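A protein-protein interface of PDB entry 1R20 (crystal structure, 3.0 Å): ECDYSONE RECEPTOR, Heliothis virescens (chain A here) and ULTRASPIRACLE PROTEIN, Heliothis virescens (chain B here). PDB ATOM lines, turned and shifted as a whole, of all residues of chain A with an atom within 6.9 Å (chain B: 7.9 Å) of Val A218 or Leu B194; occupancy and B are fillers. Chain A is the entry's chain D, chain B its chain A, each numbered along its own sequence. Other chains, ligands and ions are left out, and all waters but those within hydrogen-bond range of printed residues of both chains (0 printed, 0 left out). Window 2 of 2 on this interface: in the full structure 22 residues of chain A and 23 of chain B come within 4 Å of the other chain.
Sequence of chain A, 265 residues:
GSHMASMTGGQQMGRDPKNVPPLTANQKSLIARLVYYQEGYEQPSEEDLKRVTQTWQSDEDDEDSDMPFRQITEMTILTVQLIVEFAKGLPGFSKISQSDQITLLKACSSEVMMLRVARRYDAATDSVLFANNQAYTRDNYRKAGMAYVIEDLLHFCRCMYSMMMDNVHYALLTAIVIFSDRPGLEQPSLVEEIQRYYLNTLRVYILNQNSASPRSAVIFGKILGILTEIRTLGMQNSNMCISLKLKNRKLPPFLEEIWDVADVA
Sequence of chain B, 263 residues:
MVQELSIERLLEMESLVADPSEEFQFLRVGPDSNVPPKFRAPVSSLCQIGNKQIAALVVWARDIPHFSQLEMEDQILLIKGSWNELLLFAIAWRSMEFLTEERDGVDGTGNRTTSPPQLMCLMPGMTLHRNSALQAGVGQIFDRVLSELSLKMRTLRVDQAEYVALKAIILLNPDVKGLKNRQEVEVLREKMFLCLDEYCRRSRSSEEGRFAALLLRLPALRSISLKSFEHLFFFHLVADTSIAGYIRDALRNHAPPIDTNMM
OD2 of Asp B197 lies within salt-bridge range of NH1 of Arg B201 (3.6 Å).
Among the printed residues, pairs that only touch across the chains: Ala A217 with Asp B197 (3.4 Å), Ala A217 with Phe B211 (3.8 Å), Val A218 with Glu B190 (3.3 Å), Val A218 with Leu B194 (3.3 Å), Phe A220 with Phe B211 (3.9 Å), Gly A221 with Phe B193 (3.8 Å) and Lys A222 with Phe B193 (3.8 Å).
OE2 of Glu B190 is in salt-bridge range of NZ of Lys A222, at 3.4 Å. OE2 of Glu B186 is in salt-bridge range of NZ of Lys A222, at 2.6 Å.
Of the 12 printed residues of chain A, 5 touch a printed residue of chain B. Hydrophobic or aromatic side chains of chain A within 4 Å of the printed part of chain B: Ala A217, Val A218 and Phe A220. Of the 19 printed residues of chain B, 6 touch a printed residue of chain A. Hydrophobic or aromatic side chains of chain B within 4 Å of the printed part of chain A: Phe B193, Leu B194 and Phe B211. Among the printed residues, Asp or Glu carboxylates within 4 Å of a Lys or Arg side-chain nitrogen of the other chain: Lys A222 with Glu B186 and Lys A222 with Glu B190.
Printed residues of chain A within 4 Å of Leu B194: Val A218 (3.3 Å). Of the printed residues of chain A, Phe B211 touches Ala A217 (3.8 Å) and Phe A220 (3.9 Å). Of the printed residues of chain A, Asp B197 touches Ala A217. Of the printed residues of chain A, Glu B186 touches Lys A222 (2.6 Å). Of the printed residues of chain B, Phe A220 touches Phe B211. Of the printed residues of chain B, Gly A221 touches Phe B193. Leu B196 touches none of the printed residues of chain A. Leu B215 touches none of the printed residues of chain A. The nearest residue of chain B that does not touch Val A218 is Phe B193 (4.1 Å). The nearest residue of chain A that does not touch Leu B194 is Pro A214 (4.1 Å).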
ATOM      1  N   MET A 163       1.179   3.557   6.479  1.00  0.00           N
ATOM      2  CA  MET A 163       1.398   2.116   6.624  1.00  0.00           C
ATOM      3  C   MET A 163       2.809   1.685   6.870  1.00  0.00           C
ATOM      4  O   MET A 163       3.064   0.502   7.091  1.00  0.00           O
ATOM      5  CB  MET A 163       0.983   1.364   5.392  1.00  0.00           C
ATOM      6  CG  MET A 163      -0.076   1.992   4.619  1.00  0.00           C
ATOM      7  SD  MET A 163      -0.589   0.728   3.487  1.00  0.00           S
ATOM      8  CE  MET A 163      -2.374   0.495   4.056  1.00  0.00           C
ATOM      9  N   ILE A 206       6.278 -10.727   4.700  1.00  0.00           N
ATOM     10  CA  ILE A 206       5.673 -10.066   5.860  1.00  0.00           C
ATOM     11  C   ILE A 206       5.413 -11.070   6.991  1.00  0.00           C
ATOM     12  O   ILE A 206       5.240 -10.659   8.147  1.00  0.00           O
ATOM     13  CB  ILE A 206       4.306  -9.286   5.548  1.00  0.00           C
ATOM     14  CG1 ILE A 206       3.138 -10.257   5.472  1.00  0.00           C
ATOM     15  CG2 ILE A 206       4.360  -8.554   4.227  1.00  0.00           C
ATOM     16  CD1 ILE A 206       2.566 -10.681   6.800  1.00  0.00           C
ATOM     17  N   PRO A 214      -0.521 -12.964  14.176  1.00  0.00           N
ATOM     18  CA  PRO A 214      -1.648 -12.842  13.233  1.00  0.00           C
ATOM     19  C   PRO A 214      -1.654 -11.486  12.506  1.00  0.00           C
ATOM     20  O   PRO A 214      -2.116 -11.399  11.368  1.00  0.00           O
ATOM     21  CB  PRO A 214      -2.878 -13.049  14.127  1.00  0.00           C
ATOM     22  CG  PRO A 214      -2.327 -13.851  15.312  1.00  0.00           C
ATOM     23  CD  PRO A 214      -1.019 -13.136  15.554  1.00  0.00           C
ATOM     24  N   ARG A 215      -1.148 -10.447  13.174  1.00  0.00           N
ATOM     25  CA  ARG A 215      -1.044  -9.121  12.574  1.00  0.00           C
ATOM     26  C   ARG A 215      -0.678  -9.231  11.083  1.00  0.00           C
ATOM     27  O   ARG A 215      -1.225  -8.525  10.236  1.00  0.00           O
ATOM     28  CB  ARG A 215       0.009  -8.309  13.285  1.00  0.00           C
ATOM     29  N   SER A 216       0.252 -10.117  10.758  1.00  0.00           N
ATOM     30  CA  SER A 216       0.664 -10.318   9.368  1.00  0.00           C
ATOM     31  C   SER A 216      -0.462 -10.182   8.329  1.00  0.00           C
ATOM     32  O   SER A 216      -0.381  -9.358   7.439  1.00  0.00           O
ATOM     33  CB  SER A 216       1.328 -11.673   9.245  1.00  0.00           C
ATOM     34  OG  SER A 216       0.427 -12.635   9.698  1.00  0.00           O
ATOM     35  N   ALA A 217      -1.523 -10.971   8.457  1.00  0.00           N
ATOM     36  CA  ALA A 217      -2.658 -10.887   7.517  1.00  0.00           C
ATOM     37  C   ALA A 217      -3.168  -9.463   7.378  1.00  0.00           C
ATOM     38  O   ALA A 217      -3.511  -9.020   6.293  1.00  0.00           O
ATOM     39  CB  ALA A 217      -3.778 -11.773   7.970  1.00  0.00           C
ATOM     40  N   VAL A 218      -3.232  -8.749   8.493  1.00  0.00           N
ATOM     41  CA  VAL A 218      -3.680  -7.352   8.482  1.00  0.00           C
ATOM     42  C   VAL A 218      -2.723  -6.479   7.645  1.00  0.00           C
ATOM     43  O   VAL A 218      -3.164  -5.643   6.822  1.00  0.00           O
ATOM     44  CB  VAL A 218      -3.758  -6.786   9.954  1.00  0.00           C
ATOM     45  CG1 VAL A 218      -3.824  -5.244   9.958  1.00  0.00           C
ATOM     46  CG2 VAL A 218      -4.971  -7.396  10.659  1.00  0.00           C
ATOM     47  N   ILE A 219      -1.419  -6.699   7.874  1.00  0.00           N
ATOM     48  CA  ILE A 219      -0.369  -5.958   7.214  1.00  0.00           C
ATOM     49  C   ILE A 219      -0.438  -6.213   5.746  1.00  0.00           C
ATOM     50  O   ILE A 219      -0.357  -5.303   4.934  1.00  0.00           O
ATOM     51  CB  ILE A 219       0.984  -6.402   7.711  1.00  0.00           C
ATOM     52  CG1 ILE A 219       1.260  -5.774   9.076  1.00  0.00           C
ATOM     53  CG2 ILE A 219       2.032  -6.042   6.710  1.00  0.00           C
ATOM     54  CD1 ILE A 219       2.663  -5.999   9.600  1.00  0.00           C
ATOM     55  N   PHE A 220      -0.586  -7.491   5.435  1.00  0.00           N
ATOM     56  CA  PHE A 220      -0.677  -8.004   4.082  1.00  0.00           C
ATOM     57  C   PHE A 220      -1.950  -7.441   3.492  1.00  0.00           C
ATOM     58  O   PHE A 220      -1.975  -6.970   2.360  1.00  0.00           O
ATOM     59  CB  PHE A 220      -0.720  -9.532   4.150  1.00  0.00           C
ATOM     60  CG  PHE A 220      -0.700 -10.192   2.840  1.00  0.00           C
ATOM     61  CD1 PHE A 220       0.233  -9.825   1.886  1.00  0.00           C
ATOM     62  CD2 PHE A 220      -1.645 -11.161   2.531  1.00  0.00           C
ATOM     63  CE1 PHE A 220       0.225 -10.405   0.619  1.00  0.00           C
ATOM     64  CE2 PHE A 220      -1.670 -11.751   1.275  1.00  0.00           C
ATOM     65  CZ  PHE A 220      -0.732 -11.370   0.309  1.00  0.00           C
ATOM     66  N   GLY A 221      -3.009  -7.455   4.287  1.00  0.00           N
ATOM     67  CA  GLY A 221      -4.275  -6.939   3.811  1.00  0.00           C
ATOM     68  C   GLY A 221      -4.227  -5.486   3.377  1.00  0.00           C
ATOM     69  O   GLY A 221      -4.614  -5.182   2.252  1.00  0.00           O
ATOM     70  N   LYS A 222      -3.769  -4.604   4.272  1.00  0.00           N
ATOM     71  CA  LYS A 222      -3.655  -3.179   4.009  1.00  0.00           C
ATOM     72  C   LYS A 222      -2.860  -2.898   2.734  1.00  0.00           C
ATOM     73  O   LYS A 222      -3.088  -1.901   2.062  1.00  0.00           O
ATOM     74  CB  LYS A 222      -3.012  -2.511   5.206  1.00  0.00           C
ATOM     75  CG  LYS A 222      -3.770  -2.746   6.493  1.00  0.00           C
ATOM     76  CD  LYS A 222      -3.041  -2.151   7.690  1.00  0.00           C
ATOM     77  CE  LYS A 222      -2.699  -0.680   7.491  1.00  0.00           C
ATOM     78  NZ  LYS A 222      -3.410   0.135   8.525  1.00  0.00           N
ATOM     79  N   ILE A 223      -1.926  -3.783   2.398  1.00  0.00           N
ATOM     80  CA  ILE A 223      -1.168  -3.612   1.172  1.00  0.00           C
ATOM     81  C   ILE A 223      -2.095  -3.901  -0.006  1.00  0.00           C
ATOM     82  O   ILE A 223      -2.385  -3.017  -0.779  1.00  0.00           O
ATOM     83  CB  ILE A 223       0.095  -4.482   1.130  1.00  0.00           C
ATOM     84  CG1 ILE A 223       0.978  -4.092   2.299  1.00  0.00           C
ATOM     85  CG2 ILE A 223       0.888  -4.213  -0.149  1.00  0.00           C
ATOM     86  CD1 ILE A 223       2.411  -4.611   2.228  1.00  0.00           C
ATOM     87  N   ILE B 169     -15.618  -5.484   4.574  1.00  0.00           N
ATOM     88  CA  ILE B 169     -14.385  -4.824   4.160  1.00  0.00           C
ATOM     89  C   ILE B 169     -14.577  -3.613   3.193  1.00  0.00           C
ATOM     90  O   ILE B 169     -13.906  -2.590   3.340  1.00  0.00           O
ATOM     91  CB  ILE B 169     -13.417  -5.848   3.486  1.00  0.00           C
ATOM     92  CG1 ILE B 169     -12.943  -6.837   4.555  1.00  0.00           C
ATOM     93  CG2 ILE B 169     -12.276  -5.105   2.713  1.00  0.00           C
ATOM     94  CD1 ILE B 169     -11.709  -7.554   4.223  1.00  0.00           C
ATOM     95  N   GLU B 186     -10.186   2.058  10.863  1.00  0.00           N
ATOM     96  CA  GLU B 186      -9.104   1.222  10.434  1.00  0.00           C
ATOM     97  C   GLU B 186      -9.195  -0.043  11.274  1.00  0.00           C
ATOM     98  O   GLU B 186      -9.117  -1.151  10.748  1.00  0.00           O
ATOM     99  CB  GLU B 186      -7.779   1.902  10.670  1.00  0.00           C
ATOM    100  CG  GLU B 186      -7.304   2.677   9.485  1.00  0.00           C
ATOM    101  CD  GLU B 186      -5.788   2.711   9.422  1.00  0.00           C
ATOM    102  OE1 GLU B 186      -5.177   3.378  10.297  1.00  0.00           O
ATOM    103  OE2 GLU B 186      -5.228   2.048   8.501  1.00  0.00           O
ATOM    104  N   VAL B 187      -9.382   0.127  12.582  1.00  0.00           N
ATOM    105  CA  VAL B 187      -9.476  -1.012  13.472  1.00  0.00           C
ATOM    106  C   VAL B 187     -10.560  -1.972  13.064  1.00  0.00           C
ATOM    107  O   VAL B 187     -10.323  -3.173  13.070  1.00  0.00           O
ATOM    108  CB  VAL B 187      -9.729  -0.627  14.907  1.00  0.00           C
ATOM    109  CG1 VAL B 187     -10.846   0.394  15.012  1.00  0.00           C
ATOM    110  CG2 VAL B 187     -10.116  -1.875  15.648  1.00  0.00           C
ATOM    111  N   LEU B 188     -11.750  -1.466  12.737  1.00  0.00           N
ATOM    112  CA  LEU B 188     -12.814  -2.347  12.288  1.00  0.00           C
ATOM    113  C   LEU B 188     -12.278  -3.056  11.067  1.00  0.00           C
ATOM    114  O   LEU B 188     -12.157  -4.257  11.096  1.00  0.00           O
ATOM    115  CB  LEU B 188     -14.076  -1.582  11.929  1.00  0.00           C
ATOM    116  CG  LEU B 188     -14.811  -0.875  13.080  1.00  0.00           C
ATOM    117  CD1 LEU B 188     -15.830   0.020  12.454  1.00  0.00           C
ATOM    118  CD2 LEU B 188     -15.505  -1.826  14.048  1.00  0.00           C
ATOM    119  N   ARG B 189     -11.897  -2.347  10.007  1.00  0.00           N
ATOM    120  CA  ARG B 189     -11.387  -3.057   8.834  1.00  0.00           C
ATOM    121  C   ARG B 189     -10.392  -4.124   9.204  1.00  0.00           C
ATOM    122  O   ARG B 189     -10.483  -5.227   8.728  1.00  0.00           O
ATOM    123  CB  ARG B 189     -10.741  -2.121   7.822  1.00  0.00           C
ATOM    124  CG  ARG B 189      -9.825  -2.865   6.867  1.00  0.00           C
ATOM    125  CD  ARG B 189      -9.453  -2.064   5.634  1.00  0.00           C
ATOM    126  NE  ARG B 189     -10.578  -1.968   4.698  1.00  0.00           N
ATOM    127  CZ  ARG B 189     -10.478  -1.599   3.419  1.00  0.00           C
ATOM    128  NH1 ARG B 189      -9.315  -1.278   2.881  1.00  0.00           N
ATOM    129  NH2 ARG B 189     -11.544  -1.568   2.666  1.00  0.00           N
ATOM    130  N   GLU B 190      -9.445  -3.804  10.069  1.00  0.00           N
ATOM    131  CA  GLU B 190      -8.447  -4.786  10.470  1.00  0.00           C
ATOM    132  C   GLU B 190      -9.075  -5.961  11.170  1.00  0.00           C
ATOM    133  O   GLU B 190      -8.606  -7.073  11.065  1.00  0.00           O
ATOM    134  CB  GLU B 190      -7.413  -4.172  11.400  1.00  0.00           C
ATOM    135  CG  GLU B 190      -6.793  -2.894  10.846  1.00  0.00           C
ATOM    136  CD  GLU B 190      -5.488  -2.503  11.534  1.00  0.00           C
ATOM    137  OE1 GLU B 190      -5.428  -2.556  12.800  1.00  0.00           O
ATOM    138  OE2 GLU B 190      -4.536  -2.134  10.784  1.00  0.00           O
ATOM    139  N   LYS B 191     -10.131  -5.718  11.912  1.00  0.00           N
ATOM    140  CA  LYS B 191     -10.788  -6.814  12.588  1.00  0.00           C
ATOM    141  C   LYS B 191     -11.397  -7.753  11.542  1.00  0.00           C
ATOM    142  O   LYS B 191     -11.644  -8.917  11.817  1.00  0.00           O
ATOM    143  CB  LYS B 191     -11.872  -6.273  13.544  1.00  0.00           C
ATOM    144  CG  LYS B 191     -12.604  -7.341  14.343  1.00  0.00           C
ATOM    145  CD  LYS B 191     -11.642  -8.299  15.047  1.00  0.00           C
ATOM    146  CE  LYS B 191     -12.378  -9.268  15.932  1.00  0.00           C
ATOM    147  NZ  LYS B 191     -13.448  -9.854  15.138  1.00  0.00           N
ATOM    148  N   MET B 192     -11.612  -7.263  10.333  1.00  0.00           N
ATOM    149  CA  MET B 192     -12.210  -8.090   9.308  1.00  0.00           C
ATOM    150  C   MET B 192     -11.193  -8.831   8.504  1.00  0.00           C
ATOM    151  O   MET B 192     -11.546  -9.786   7.831  1.00  0.00           O
ATOM    152  CB  MET B 192     -13.041  -7.257   8.349  1.00  0.00           C
ATOM    153  CG  MET B 192     -14.352  -6.729   8.895  1.00  0.00           C
ATOM    154  SD  MET B 192     -15.405  -8.054   9.443  1.00  0.00           S
ATOM    155  CE  MET B 192     -15.193  -9.351   8.098  1.00  0.00           C
ATOM    156  N   PHE B 193      -9.943  -8.365   8.515  1.00  0.00           N
ATOM    157  CA  PHE B 193      -8.864  -9.044   7.782  1.00  0.00           C
ATOM    158  C   PHE B 193      -8.460 -10.218   8.651  1.00  0.00           C
ATOM    159  O   PHE B 193      -8.162 -11.323   8.164  1.00  0.00           O
ATOM    160  CB  PHE B 193      -7.643  -8.145   7.587  1.00  0.00           C
ATOM    161  CG  PHE B 193      -7.760  -7.176   6.440  1.00  0.00           C
ATOM    162  CD1 PHE B 193      -8.325  -7.552   5.246  1.00  0.00           C
ATOM    163  CD2 PHE B 193      -7.267  -5.888   6.551  1.00  0.00           C
ATOM    164  CE1 PHE B 193      -8.396  -6.667   4.192  1.00  0.00           C
ATOM    165  CE2 PHE B 193      -7.340  -5.000   5.486  1.00  0.00           C
ATOM    166  CZ  PHE B 193      -7.900  -5.392   4.319  1.00  0.00           C
ATOM    167  N   LEU B 194      -8.453  -9.973   9.959  1.00  0.00           N
ATOM    168  CA  LEU B 194      -8.108 -11.013  10.906  1.00  0.00           C
ATOM    169  C   LEU B 194      -9.165 -12.090  10.775  1.00  0.00           C
ATOM    170  O   LEU B 194      -8.821 -13.260  10.688  1.00  0.00           O
ATOM    171  CB  LEU B 194      -8.044 -10.471  12.342  1.00  0.00           C
ATOM    172  CG  LEU B 194      -6.740 -10.859  13.062  1.00  0.00           C
ATOM    173  CD1 LEU B 194      -5.668  -9.798  12.767  1.00  0.00           C
ATOM    174  CD2 LEU B 194      -6.958 -10.988  14.583  1.00  0.00           C
ATOM    175  N   CYS B 195     -10.440 -11.716  10.722  1.00  0.00           N
ATOM    176  CA  CYS B 195     -11.482 -12.723  10.583  1.00  0.00           C
ATOM    177  C   CYS B 195     -11.382 -13.486   9.285  1.00  0.00           C
ATOM    178  O   CYS B 195     -11.447 -14.706   9.273  1.00  0.00           O
ATOM    179  CB  CYS B 195     -12.860 -12.096  10.624  1.00  0.00           C
ATOM    180  SG  CYS B 195     -13.245 -11.374  12.194  1.00  0.00           S
ATOM    181  N   LEU B 196     -11.237 -12.748   8.194  1.00  0.00           N
ATOM    182  CA  LEU B 196     -11.174 -13.295   6.858  1.00  0.00           C
ATOM    183  C   LEU B 196     -10.008 -14.247   6.599  1.00  0.00           C
ATOM    184  O   LEU B 196     -10.131 -15.225   5.849  1.00  0.00           O
ATOM    185  CB  LEU B 196     -11.114 -12.145   5.876  1.00  0.00           C
ATOM    186  CG  LEU B 196     -10.960 -12.751   4.500  1.00  0.00           C
ATOM    187  CD1 LEU B 196     -12.205 -13.588   4.250  1.00  0.00           C
ATOM    188  CD2 LEU B 196     -10.703 -11.684   3.445  1.00  0.00           C
ATOM    189  N   ASP B 197      -8.867 -13.928   7.201  1.00  0.00           N
ATOM    190  CA  ASP B 197      -7.669 -14.728   7.055  1.00  0.00           C
ATOM    191  C   ASP B 197      -7.794 -16.010   7.859  1.00  0.00           C
ATOM    192  O   ASP B 197      -7.439 -17.077   7.396  1.00  0.00           O
ATOM    193  CB  ASP B 197      -6.462 -13.969   7.577  1.00  0.00           C
ATOM    194  CG  ASP B 197      -5.232 -14.881   7.749  1.00  0.00           C
ATOM    195  OD1 ASP B 197      -4.605 -15.232   6.703  1.00  0.00           O
ATOM    196  OD2 ASP B 197      -4.915 -15.248   8.922  1.00  0.00           O
ATOM    197  N   GLU B 198      -8.252 -15.875   9.095  1.00  0.00           N
ATOM    198  CA  GLU B 198      -8.453 -17.000   9.976  1.00  0.00           C
ATOM    199  C   GLU B 198      -9.455 -17.911   9.308  1.00  0.00           C
ATOM    200  O   GLU B 198      -9.119 -19.011   8.948  1.00  0.00           O
ATOM    201  CB  GLU B 198      -9.005 -16.516  11.299  1.00  0.00           C
ATOM    202  CG  GLU B 198      -9.482 -17.600  12.206  1.00  0.00           C
ATOM    203  CD  GLU B 198     -10.617 -17.112  13.093  1.00  0.00           C
ATOM    204  OE1 GLU B 198     -10.559 -15.942  13.552  1.00  0.00           O
ATOM    205  OE2 GLU B 198     -11.565 -17.899  13.338  1.00  0.00           O
ATOM    206  N   TYR B 199     -10.689 -17.470   9.133  1.00  0.00           N
ATOM    207  CA  TYR B 199     -11.654 -18.332   8.477  1.00  0.00           C
ATOM    208  C   TYR B 199     -10.979 -19.077   7.314  1.00  0.00           C
ATOM    209  O   TYR B 199     -10.896 -20.297   7.327  1.00  0.00           O
ATOM    210  CB  TYR B 199     -12.835 -17.513   7.964  1.00  0.00           C
ATOM    211  CG  TYR B 199     -13.732 -18.262   7.001  1.00  0.00           C
ATOM    212  CD1 TYR B 199     -14.991 -18.706   7.389  1.00  0.00           C
ATOM    213  CD2 TYR B 199     -13.305 -18.549   5.706  1.00  0.00           C
ATOM    214  CE1 TYR B 199     -15.803 -19.425   6.510  1.00  0.00           C
ATOM    215  CE2 TYR B 199     -14.100 -19.261   4.825  1.00  0.00           C
ATOM    216  CZ  TYR B 199     -15.348 -19.700   5.229  1.00  0.00           C
ATOM    217  OH  TYR B 199     -16.116 -20.438   4.349  1.00  0.00           O
ATOM    218  N   CYS B 200     -10.483 -18.336   6.326  1.00  0.00           N
ATOM    219  CA  CYS B 200      -9.815 -18.905   5.154  1.00  0.00           C
ATOM    220  C   CYS B 200      -8.825 -20.041   5.346  1.00  0.00           C
ATOM    221  O   CYS B 200      -8.598 -20.823   4.431  1.00  0.00           O
ATOM    222  CB  CYS B 200      -9.106 -17.810   4.381  1.00  0.00           C
ATOM    223  SG  CYS B 200     -10.155 -17.045   3.199  1.00  0.00           S
ATOM    224  N   ARG B 201      -8.192 -20.125   6.502  1.00  0.00           N
ATOM    225  CA  ARG B 201      -7.256 -21.212   6.703  1.00  0.00           C
ATOM    226  C   ARG B 201      -8.035 -22.342   7.349  1.00  0.00           C
ATOM    227  O   ARG B 201      -8.025 -23.469   6.867  1.00  0.00           O
ATOM    228  CB  ARG B 201      -6.064 -20.776   7.577  1.00  0.00           C
ATOM    229  CG  ARG B 201      -6.384 -20.461   9.032  1.00  0.00           C
ATOM    230  CD  ARG B 201      -5.300 -19.590   9.701  1.00  0.00           C
ATOM    231  NE  ARG B 201      -5.816 -18.923  10.903  1.00  0.00           N
ATOM    232  CZ  ARG B 201      -5.128 -18.067  11.652  1.00  0.00           C
ATOM    233  NH1 ARG B 201      -3.875 -17.769  11.331  1.00  0.00           N
ATOM    234  NH2 ARG B 201      -5.703 -17.500  12.712  1.00  0.00           N
ATOM    235  N   PHE B 211      -6.711 -16.000   0.747  1.00  0.00           N
ATOM    236  CA  PHE B 211      -6.922 -14.718   1.339  1.00  0.00           C
ATOM    237  C   PHE B 211      -6.609 -13.601   0.410  1.00  0.00           C
ATOM    238  O   PHE B 211      -7.228 -12.559   0.524  1.00  0.00           O
ATOM    239  CB  PHE B 211      -6.082 -14.543   2.555  1.00  0.00           C
ATOM    240  CG  PHE B 211      -6.275 -13.237   3.211  1.00  0.00           C
ATOM    241  CD1 PHE B 211      -7.403 -12.987   3.952  1.00  0.00           C
ATOM    242  CD2 PHE B 211      -5.325 -12.260   3.105  1.00  0.00           C
ATOM    243  CE1 PHE B 211      -7.581 -11.778   4.587  1.00  0.00           C
ATOM    244  CE2 PHE B 211      -5.490 -11.068   3.726  1.00  0.00           C
ATOM    245  CZ  PHE B 211      -6.624 -10.818   4.477  1.00  0.00           C
ATOM    246  N   LEU B 215      -9.175 -10.858  -1.886  1.00  0.00           N
ATOM    247  CA  LEU B 215      -8.945  -9.456  -1.772  1.00  0.00           C
ATOM    248  C   LEU B 215      -8.637  -8.777  -3.107  1.00  0.00           C
ATOM    249  O   LEU B 215      -8.643  -7.534  -3.201  1.00  0.00           O
ATOM    250  CB  LEU B 215      -7.839  -9.252  -0.771  1.00  0.00           C
ATOM    251  CG  LEU B 215      -8.469  -9.280   0.610  1.00  0.00           C
ATOM    252  CD1 LEU B 215      -7.444  -8.913   1.655  1.00  0.00           C
ATOM    253  CD2 LEU B 215      -9.599  -8.273   0.683  1.00  0.00           C
